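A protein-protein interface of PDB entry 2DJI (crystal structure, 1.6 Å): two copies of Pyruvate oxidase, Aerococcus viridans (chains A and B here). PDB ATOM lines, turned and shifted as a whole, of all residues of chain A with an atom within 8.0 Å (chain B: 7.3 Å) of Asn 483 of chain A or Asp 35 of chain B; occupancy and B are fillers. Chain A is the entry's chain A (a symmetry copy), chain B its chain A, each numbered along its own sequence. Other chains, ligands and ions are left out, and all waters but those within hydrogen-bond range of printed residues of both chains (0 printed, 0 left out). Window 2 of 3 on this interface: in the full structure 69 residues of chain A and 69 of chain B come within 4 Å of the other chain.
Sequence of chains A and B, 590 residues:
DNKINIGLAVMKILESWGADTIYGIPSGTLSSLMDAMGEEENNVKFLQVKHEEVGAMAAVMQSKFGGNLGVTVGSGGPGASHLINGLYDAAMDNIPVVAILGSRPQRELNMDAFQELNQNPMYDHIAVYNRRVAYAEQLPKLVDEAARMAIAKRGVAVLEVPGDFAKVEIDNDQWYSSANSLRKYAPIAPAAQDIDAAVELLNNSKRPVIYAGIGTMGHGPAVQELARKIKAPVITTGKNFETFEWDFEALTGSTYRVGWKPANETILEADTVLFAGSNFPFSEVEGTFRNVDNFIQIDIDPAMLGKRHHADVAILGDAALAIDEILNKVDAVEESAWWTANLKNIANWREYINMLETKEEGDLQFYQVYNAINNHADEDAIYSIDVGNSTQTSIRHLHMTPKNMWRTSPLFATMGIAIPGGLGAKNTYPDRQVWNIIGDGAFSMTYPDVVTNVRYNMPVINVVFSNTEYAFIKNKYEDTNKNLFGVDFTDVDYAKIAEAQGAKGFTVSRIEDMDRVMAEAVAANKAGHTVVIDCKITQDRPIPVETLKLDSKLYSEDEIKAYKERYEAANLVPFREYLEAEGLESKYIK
O of Ser 27 of chain B sits at hydrogen-bond distance from OH of Tyr 477 of chain A. OG of Ser 31 of chain B lies close to ND2 of Asn 481 of chain A, at 3.0 Å. The side-chain amide nitrogen of Asn 481 of chain A lies within hydrogen-bond range of the side-chain carboxylate of Asp 35 of chain B.
The side-chain carboxylate (OD1) of Asp 35 of chain B sits close to the backbone carbonyl oxygen (O) of Ser 31 of chain B (2.5 Å). The side-chain hydroxyl (OG1) of Thr 480 of chain A lies within hydrogen-bond range of the side-chain amide oxygen (OD1) of Asn 481 of chain A (2.8 Å).
Among the printed residues, pairs that only touch across the chains: Tyr 477 of chain A with Met 34 of chain B (3.1 Å), Tyr 477 of chain A with Ser 31 of chain B (3.3 Å), Asn 483 of chain A with Asp 35 of chain B (3.5 Å), Leu 484 of chain A with Asp 35 of chain B (3.6 Å), Asn 481 of chain A with Ser 32 of chain B (3.8 Å) and Tyr 477 of chain A with Asp 35 of chain B (3.9 Å).
Of the printed residues of chain B, Asn 483 of chain A touches Asp 35 (3.5 Å). Asp 35 of chain B touches four residues of chain A. Of the printed residues of chain A, Met 34 of chain B touches Tyr 477 (3.1 Å). Of the printed residues of chain A, Ser 31 of chain B touches Tyr 477 and Asn 481. Of the printed residues of chain A, Ser 27 of chain B touches Tyr 477 (3.4 Å). Asp 479 of chain A touches none of the printed residues of chain B. The nearest residue of chain A that does not touch Asp 35 of chain B is Lys 482 of chain A (4.2 Å).
Of the 16 printed residues of chain B, 5 touch a printed residue of chain A. Printed residues of chain A that touch a printed residue of chain B: Tyr 477, Asn 481, Asn 483 and Leu 484. Along chain A the printed residues that touch a printed residue of chain B span positions 477 to 484. Among the printed residues, 9 pairs touch across the chains. Among the printed residues, no Asp or Glu carboxylate lies within 4 Å of a Lys or Arg side-chain nitrogen of the other chain.
No position is printed for both chains. Of the 9 pairs that touch across the chains among the printed residues, none has its exchanged pair printed and touching as well.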
ATOM      1  N   LYS A 474      -5.530 -22.581 -24.694  1.00  0.00           N
ATOM      2  CA  LYS A 474      -5.722 -23.655 -23.725  1.00  0.00           C
ATOM      3  C   LYS A 474      -4.791 -23.518 -22.521  1.00  0.00           C
ATOM      4  O   LYS A 474      -5.123 -23.955 -21.418  1.00  0.00           O
ATOM      5  CB  LYS A 474      -5.494 -25.010 -24.402  1.00  0.00           C
ATOM      6  CG  LYS A 474      -5.734 -26.211 -23.503  1.00  0.00           C
ATOM      7  CD  LYS A 474      -5.509 -27.512 -24.258  1.00  0.00           C
ATOM      8  CE  LYS A 474      -5.786 -28.722 -23.380  1.00  0.00           C
ATOM      9  NZ  LYS A 474      -5.592 -30.003 -24.116  1.00  0.00           N
ATOM     10  N   LYS A 476      -3.800 -20.656 -21.119  1.00  0.00           N
ATOM     11  CA  LYS A 476      -4.305 -19.613 -20.232  1.00  0.00           C
ATOM     12  C   LYS A 476      -5.532 -20.095 -19.463  1.00  0.00           C
ATOM     13  O   LYS A 476      -5.750 -19.694 -18.318  1.00  0.00           O
ATOM     14  CB  LYS A 476      -4.652 -18.355 -21.035  1.00  0.00           C
ATOM     15  CG  LYS A 476      -5.310 -17.248 -20.215  1.00  0.00           C
ATOM     16  CD  LYS A 476      -4.457 -16.830 -19.022  1.00  0.00           C
ATOM     17  CE  LYS A 476      -3.137 -16.215 -19.457  1.00  0.00           C
ATOM     18  NZ  LYS A 476      -2.315 -15.770 -18.295  1.00  0.00           N
ATOM     19  N   TYR A 477      -6.330 -20.952 -20.095  1.00  0.00           N
ATOM     20  CA  TYR A 477      -7.531 -21.495 -19.463  1.00  0.00           C
ATOM     21  C   TYR A 477      -7.224 -22.053 -18.080  1.00  0.00           C
ATOM     22  O   TYR A 477      -7.944 -21.789 -17.118  1.00  0.00           O
ATOM     23  CB  TYR A 477      -8.132 -22.609 -20.326  1.00  0.00           C
ATOM     24  CG  TYR A 477      -9.036 -22.128 -21.439  1.00  0.00           C
ATOM     25  CD1 TYR A 477      -8.613 -21.155 -22.342  1.00  0.00           C
ATOM     26  CD2 TYR A 477     -10.311 -22.670 -21.606  1.00  0.00           C
ATOM     27  CE1 TYR A 477      -9.435 -20.733 -23.385  1.00  0.00           C
ATOM     28  CE2 TYR A 477     -11.140 -22.257 -22.645  1.00  0.00           C
ATOM     29  CZ  TYR A 477     -10.695 -21.289 -23.531  1.00  0.00           C
ATOM     30  OH  TYR A 477     -11.508 -20.878 -24.562  1.00  0.00           O
ATOM     31  N   GLU A 478      -6.146 -22.826 -17.987  1.00  0.00           N
ATOM     32  CA  GLU A 478      -5.732 -23.438 -16.729  1.00  0.00           C
ATOM     33  C   GLU A 478      -5.508 -22.407 -15.625  1.00  0.00           C
ATOM     34  O   GLU A 478      -5.265 -22.766 -14.473  1.00  0.00           O
ATOM     35  CB  GLU A 478      -4.452 -24.246 -16.945  1.00  0.00           C
ATOM     36  CG  GLU A 478      -4.574 -25.316 -18.016  1.00  0.00           C
ATOM     37  CD  GLU A 478      -3.254 -25.999 -18.306  1.00  0.00           C
ATOM     38  OE1 GLU A 478      -2.298 -25.299 -18.703  1.00  0.00           O
ATOM     39  OE2 GLU A 478      -3.174 -27.234 -18.140  1.00  0.00           O
ATOM     40  N   ASP A 479      -5.592 -21.129 -15.981  1.00  0.00           N
ATOM     41  CA  ASP A 479      -5.393 -20.052 -15.017  1.00  0.00           C
ATOM     42  C   ASP A 479      -6.650 -19.205 -14.843  1.00  0.00           C
ATOM     43  O   ASP A 479      -7.291 -19.241 -13.793  1.00  0.00           O
ATOM     44  CB  ASP A 479      -4.233 -19.160 -15.464  1.00  0.00           C
ATOM     45  CG  ASP A 479      -2.947 -19.935 -15.666  1.00  0.00           C
ATOM     46  OD1 ASP A 479      -2.463 -20.552 -14.692  1.00  0.00           O
ATOM     47  OD2 ASP A 479      -2.420 -19.929 -16.799  1.00  0.00           O
ATOM     48  N   THR A 480      -6.996 -18.446 -15.879  1.00  0.00           N
ATOM     49  CA  THR A 480      -8.171 -17.584 -15.840  1.00  0.00           C
ATOM     50  C   THR A 480      -9.475 -18.374 -15.886  1.00  0.00           C
ATOM     51  O   THR A 480     -10.549 -17.828 -15.628  1.00  0.00           O
ATOM     52  CB  THR A 480      -8.166 -16.585 -17.016  1.00  0.00           C
ATOM     53  OG1 THR A 480      -8.139 -17.302 -18.255  1.00  0.00           O
ATOM     54  CG2 THR A 480      -6.948 -15.676 -16.935  1.00  0.00           C
ATOM     55  N   ASN A 481      -9.381 -19.659 -16.213  1.00  0.00           N
ATOM     56  CA  ASN A 481     -10.562 -20.510 -16.288  1.00  0.00           C
ATOM     57  C   ASN A 481     -10.470 -21.707 -15.345  1.00  0.00           C
ATOM     58  O   ASN A 481      -9.410 -22.313 -15.193  1.00  0.00           O
ATOM     59  CB  ASN A 481     -10.768 -21.005 -17.722  1.00  0.00           C
ATOM     60  CG  ASN A 481     -11.048 -19.875 -18.693  1.00  0.00           C
ATOM     61  OD1 ASN A 481     -10.201 -19.009 -18.916  1.00  0.00           O
ATOM     62  ND2 ASN A 481     -12.241 -19.877 -19.275  1.00  0.00           N
ATOM     63  N   LYS A 482     -11.591 -22.035 -14.713  1.00  0.00           N
ATOM     64  CA  LYS A 482     -11.652 -23.161 -13.790  1.00  0.00           C
ATOM     65  C   LYS A 482     -12.121 -24.398 -14.546  1.00  0.00           C
ATOM     66  O   LYS A 482     -12.552 -25.384 -13.946  1.00  0.00           O
ATOM     67  CB  LYS A 482     -12.618 -22.849 -12.646  1.00  0.00           C
ATOM     68  CG  LYS A 482     -12.270 -21.587 -11.873  1.00  0.00           C
ATOM     69  CD  LYS A 482     -13.307 -21.282 -10.804  1.00  0.00           C
ATOM     70  CE  LYS A 482     -12.972 -19.994 -10.068  1.00  0.00           C
ATOM     71  NZ  LYS A 482     -13.989 -19.659  -9.033  1.00  0.00           N
ATOM     72  N   ASN A 483     -12.032 -24.333 -15.871  1.00  0.00           N
ATOM     73  CA  ASN A 483     -12.444 -25.433 -16.733  1.00  0.00           C
ATOM     74  C   ASN A 483     -11.592 -25.432 -18.004  1.00  0.00           C
ATOM     75  O   ASN A 483     -10.378 -25.231 -17.944  1.00  0.00           O
ATOM     76  CB  ASN A 483     -13.929 -25.288 -17.087  1.00  0.00           C
ATOM     77  CG  ASN A 483     -14.479 -26.496 -17.822  1.00  0.00           C
ATOM     78  OD1 ASN A 483     -14.444 -27.616 -17.314  1.00  0.00           O
ATOM     79  ND2 ASN A 483     -14.993 -26.272 -19.027  1.00  0.00           N
ATOM     80  N   LEU A 484     -12.231 -25.651 -19.149  1.00  0.00           N
ATOM     81  CA  LEU A 484     -11.534 -25.673 -20.432  1.00  0.00           C
ATOM     82  C   LEU A 484     -12.544 -25.770 -21.572  1.00  0.00           C
ATOM     83  O   LEU A 484     -13.046 -24.754 -22.053  1.00  0.00           O
ATOM     84  CB  LEU A 484     -10.566 -26.860 -20.486  1.00  0.00           C
ATOM     85  CG  LEU A 484      -9.670 -26.983 -21.721  1.00  0.00           C
ATOM     86  CD1 LEU A 484      -8.772 -25.759 -21.832  1.00  0.00           C
ATOM     87  CD2 LEU A 484      -8.833 -28.248 -21.617  1.00  0.00           C
ATOM     88  N   PHE A 485     -12.834 -26.996 -21.998  1.00  0.00           N
ATOM     89  CA  PHE A 485     -13.791 -27.246 -23.073  1.00  0.00           C
ATOM     90  C   PHE A 485     -13.336 -26.745 -24.442  1.00  0.00           C
ATOM     91  O   PHE A 485     -12.888 -25.608 -24.584  1.00  0.00           O
ATOM     92  CB  PHE A 485     -15.151 -26.626 -22.715  1.00  0.00           C
ATOM     93  CG  PHE A 485     -16.135 -26.601 -23.856  1.00  0.00           C
ATOM     94  CD1 PHE A 485     -16.073 -25.607 -24.830  1.00  0.00           C
ATOM     95  CD2 PHE A 485     -17.122 -27.577 -23.959  1.00  0.00           C
ATOM     96  CE1 PHE A 485     -16.977 -25.585 -25.888  1.00  0.00           C
ATOM     97  CE2 PHE A 485     -18.033 -27.563 -25.015  1.00  0.00           C
ATOM     98  CZ  PHE A 485     -17.959 -26.564 -25.981  1.00  0.00           C
ATOM     99  N   GLY A 486     -13.465 -27.616 -25.441  1.00  0.00           N
ATOM    100  CA  GLY A 486     -13.100 -27.293 -26.810  1.00  0.00           C
ATOM    101  C   GLY A 486     -11.878 -26.421 -27.032  1.00  0.00           C
ATOM    102  O   GLY A 486     -11.890 -25.227 -26.729  1.00  0.00           O
ATOM    103  N   ASN B   5     -24.511 -18.372 -12.798  1.00  0.00           N
ATOM    104  CA  ASN B   5     -23.393 -17.779 -13.514  1.00  0.00           C
ATOM    105  C   ASN B   5     -23.962 -17.064 -14.736  1.00  0.00           C
ATOM    106  O   ASN B   5     -24.866 -17.578 -15.389  1.00  0.00           O
ATOM    107  CB  ASN B   5     -22.411 -18.876 -13.932  1.00  0.00           C
ATOM    108  CG  ASN B   5     -21.362 -18.383 -14.901  1.00  0.00           C
ATOM    109  OD1 ASN B   5     -21.481 -18.573 -16.112  1.00  0.00           O
ATOM    110  ND2 ASN B   5     -20.329 -17.737 -14.375  1.00  0.00           N
ATOM    111  N   GLY B   7     -22.641 -16.525 -17.676  1.00  0.00           N
ATOM    112  CA  GLY B   7     -22.427 -17.270 -18.902  1.00  0.00           C
ATOM    113  C   GLY B   7     -23.510 -18.321 -19.091  1.00  0.00           C
ATOM    114  O   GLY B   7     -23.985 -18.546 -20.204  1.00  0.00           O
ATOM    115  N   LEU B   8     -23.902 -18.972 -17.999  1.00  0.00           N
ATOM    116  CA  LEU B   8     -24.936 -19.999 -18.060  1.00  0.00           C
ATOM    117  C   LEU B   8     -26.306 -19.413 -18.384  1.00  0.00           C
ATOM    118  O   LEU B   8     -27.102 -20.032 -19.093  1.00  0.00           O
ATOM    119  CB  LEU B   8     -25.008 -20.764 -16.739  1.00  0.00           C
ATOM    120  CG  LEU B   8     -26.086 -21.849 -16.666  1.00  0.00           C
ATOM    121  CD1 LEU B   8     -25.884 -22.865 -17.783  1.00  0.00           C
ATOM    122  CD2 LEU B   8     -26.024 -22.528 -15.309  1.00  0.00           C
ATOM    123  N   MET B  11     -26.408 -18.947 -21.991  1.00  0.00           N
ATOM    124  CA  MET B  11     -26.646 -20.197 -22.702  1.00  0.00           C
ATOM    125  C   MET B  11     -28.108 -20.628 -22.579  1.00  0.00           C
ATOM    126  O   MET B  11     -28.683 -21.160 -23.527  1.00  0.00           O
ATOM    127  CB  MET B  11     -25.719 -21.294 -22.174  1.00  0.00           C
ATOM    128  CG  MET B  11     -24.242 -21.053 -22.469  1.00  0.00           C
ATOM    129  SD  MET B  11     -23.907 -20.808 -24.240  1.00  0.00           S
ATOM    130  CE  MET B  11     -22.653 -19.522 -24.184  1.00  0.00           C
ATOM    131  N   SER B  27     -11.015 -18.956 -27.514  1.00  0.00           N
ATOM    132  CA  SER B  27     -10.008 -17.933 -27.254  1.00  0.00           C
ATOM    133  C   SER B  27     -10.168 -17.371 -25.846  1.00  0.00           C
ATOM    134  O   SER B  27     -11.221 -17.508 -25.230  1.00  0.00           O
ATOM    135  CB  SER B  27     -10.131 -16.794 -28.267  1.00  0.00           C
ATOM    136  OG  SER B  27      -9.259 -15.726 -27.937  1.00  0.00           O
ATOM    137  N   LEU B  30     -13.110 -15.200 -24.994  1.00  0.00           N
ATOM    138  CA  LEU B  30     -14.403 -15.865 -25.157  1.00  0.00           C
ATOM    139  C   LEU B  30     -14.558 -17.056 -24.211  1.00  0.00           C
ATOM    140  O   LEU B  30     -15.648 -17.621 -24.085  1.00  0.00           O
ATOM    141  CB  LEU B  30     -14.565 -16.367 -26.597  1.00  0.00           C
ATOM    142  CG  LEU B  30     -14.713 -15.363 -27.743  1.00  0.00           C
ATOM    143  CD1 LEU B  30     -14.591 -16.098 -29.076  1.00  0.00           C
ATOM    144  CD2 LEU B  30     -16.060 -14.659 -27.643  1.00  0.00           C
ATOM    145  N   SER B  31     -13.468 -17.426 -23.545  1.00  0.00           N
ATOM    146  CA  SER B  31     -13.460 -18.576 -22.644  1.00  0.00           C
ATOM    147  C   SER B  31     -14.512 -18.583 -21.538  1.00  0.00           C
ATOM    148  O   SER B  31     -15.116 -19.620 -21.268  1.00  0.00           O
ATOM    149  CB  SER B  31     -12.065 -18.751 -22.028  1.00  0.00           C
ATOM    150  OG  SER B  31     -11.713 -17.653 -21.210  1.00  0.00           O
ATOM    151  N   SER B  32     -14.736 -17.441 -20.895  1.00  0.00           N
ATOM    152  CA  SER B  32     -15.723 -17.381 -19.820  1.00  0.00           C
ATOM    153  C   SER B  32     -17.120 -17.756 -20.296  1.00  0.00           C
ATOM    154  O   SER B  32     -17.868 -18.418 -19.576  1.00  0.00           O
ATOM    155  CB  SER B  32     -15.738 -15.989 -19.187  1.00  0.00           C
ATOM    156  OG  SER B  32     -14.542 -15.767 -18.461  1.00  0.00           O
ATOM    157  N   LEU B  33     -17.475 -17.334 -21.506  1.00  0.00           N
ATOM    158  CA  LEU B  33     -18.783 -17.664 -22.063  1.00  0.00           C
ATOM    159  C   LEU B  33     -18.843 -19.147 -22.399  1.00  0.00           C
ATOM    160  O   LEU B  33     -19.763 -19.852 -21.987  1.00  0.00           O
ATOM    161  CB  LEU B  33     -19.052 -16.858 -23.337  1.00  0.00           C
ATOM    162  CG  LEU B  33     -19.725 -15.493 -23.213  1.00  0.00           C
ATOM    163  CD1 LEU B  33     -19.804 -14.842 -24.588  1.00  0.00           C
ATOM    164  CD2 LEU B  33     -21.120 -15.664 -22.624  1.00  0.00           C
ATOM    165  N   MET B  34     -17.850 -19.613 -23.149  1.00  0.00           N
ATOM    166  CA  MET B  34     -17.783 -21.008 -23.564  1.00  0.00           C
ATOM    167  C   MET B  34     -17.742 -21.988 -22.398  1.00  0.00           C
ATOM    168  O   MET B  34     -18.276 -23.091 -22.494  1.00  0.00           O
ATOM    169  CB  MET B  34     -16.566 -21.222 -24.465  1.00  0.00           C
ATOM    170  CG  MET B  34     -16.570 -20.349 -25.708  1.00  0.00           C
ATOM    171  SD  MET B  34     -15.188 -20.706 -26.809  1.00  0.00           S
ATOM    172  CE  MET B  34     -13.894 -19.701 -26.071  1.00  0.00           C
ATOM    173  N   ASP B  35     -17.106 -21.587 -21.301  1.00  0.00           N
ATOM    174  CA  ASP B  35     -17.002 -22.438 -20.118  1.00  0.00           C
ATOM    175  C   ASP B  35     -18.371 -22.822 -19.563  1.00  0.00           C
ATOM    176  O   ASP B  35     -18.517 -23.852 -18.906  1.00  0.00           O
ATOM    177  CB  ASP B  35     -16.191 -21.728 -19.030  1.00  0.00           C
ATOM    178  CG  ASP B  35     -14.693 -21.855 -19.239  1.00  0.00           C
ATOM    179  OD1 ASP B  35     -14.247 -21.847 -20.404  1.00  0.00           O
ATOM    180  OD2 ASP B  35     -13.960 -21.949 -18.234  1.00  0.00           O
ATOM    181  N   ALA B  36     -19.371 -21.990 -19.836  1.00  0.00           N
ATOM    182  CA  ALA B  36     -20.725 -22.235 -19.353  1.00  0.00           C
ATOM    183  C   ALA B  36     -21.479 -23.241 -20.216  1.00  0.00           C
ATOM    184  O   ALA B  36     -22.425 -23.879 -19.749  1.00  0.00           O
ATOM    185  CB  ALA B  36     -21.497 -20.925 -19.289  1.00  0.00           C
ATOM    186  N   MET B  37     -21.068 -23.377 -21.473  1.00  0.00           N
ATOM    187  CA  MET B  37     -21.722 -24.309 -22.382  1.00  0.00           C
ATOM    188  C   MET B  37     -21.777 -25.692 -21.751  1.00  0.00           C
ATOM    189  O   MET B  37     -20.775 -26.197 -21.242  1.00  0.00           O
ATOM    190  CB  MET B  37     -20.983 -24.349 -23.720  1.00  0.00           C
ATOM    191  CG  MET B  37     -21.018 -23.014 -24.445  1.00  0.00           C
ATOM    192  SD  MET B  37     -20.284 -23.064 -26.077  1.00  0.00           S
ATOM    193  CE  MET B  37     -21.672 -23.625 -27.052  1.00  0.00           C
ATOM    194  N   GLY B  38     -22.955 -26.300 -21.791  1.00  0.00           N
ATOM    195  CA  GLY B  38     -23.125 -27.597 -21.169  1.00  0.00           C
ATOM    196  C   GLY B  38     -23.477 -27.265 -19.734  1.00  0.00           C
ATOM    197  O   GLY B  38     -23.822 -26.118 -19.446  1.00  0.00           O
ATOM    198  N   GLU B  39     -23.390 -28.233 -18.829  1.00  0.00           N
ATOM    199  CA  GLU B  39     -23.717 -27.977 -17.428  1.00  0.00           C
ATOM    200  C   GLU B  39     -25.179 -27.588 -17.253  1.00  0.00           C
ATOM    201  O   GLU B  39     -25.777 -26.939 -18.117  1.00  0.00           O
ATOM    202  CB  GLU B  39     -22.816 -26.875 -16.863  1.00  0.00           C
ATOM    203  CG  GLU B  39     -21.651 -27.383 -16.021  1.00  0.00           C
ATOM    204  CD  GLU B  39     -20.864 -28.487 -16.701  1.00  0.00           C
ATOM    205  OE1 GLU B  39     -21.404 -29.606 -16.848  1.00  0.00           O
ATOM    206  OE2 GLU B  39     -19.705 -28.234 -17.092  1.00  0.00           O
ATOM    207  N   ALA B 166     -18.843 -12.818 -18.216  1.00  0.00           N
ATOM    208  CA  ALA B 166     -19.472 -14.129 -18.067  1.00  0.00           C
ATOM    209  C   ALA B 166     -19.117 -14.871 -16.781  1.00  0.00           C
ATOM    210  O   ALA B 166     -19.802 -15.822 -16.406  1.00  0.00           O
ATOM    211  CB  ALA B 166     -19.145 -15.003 -19.282  1.00  0.00           C
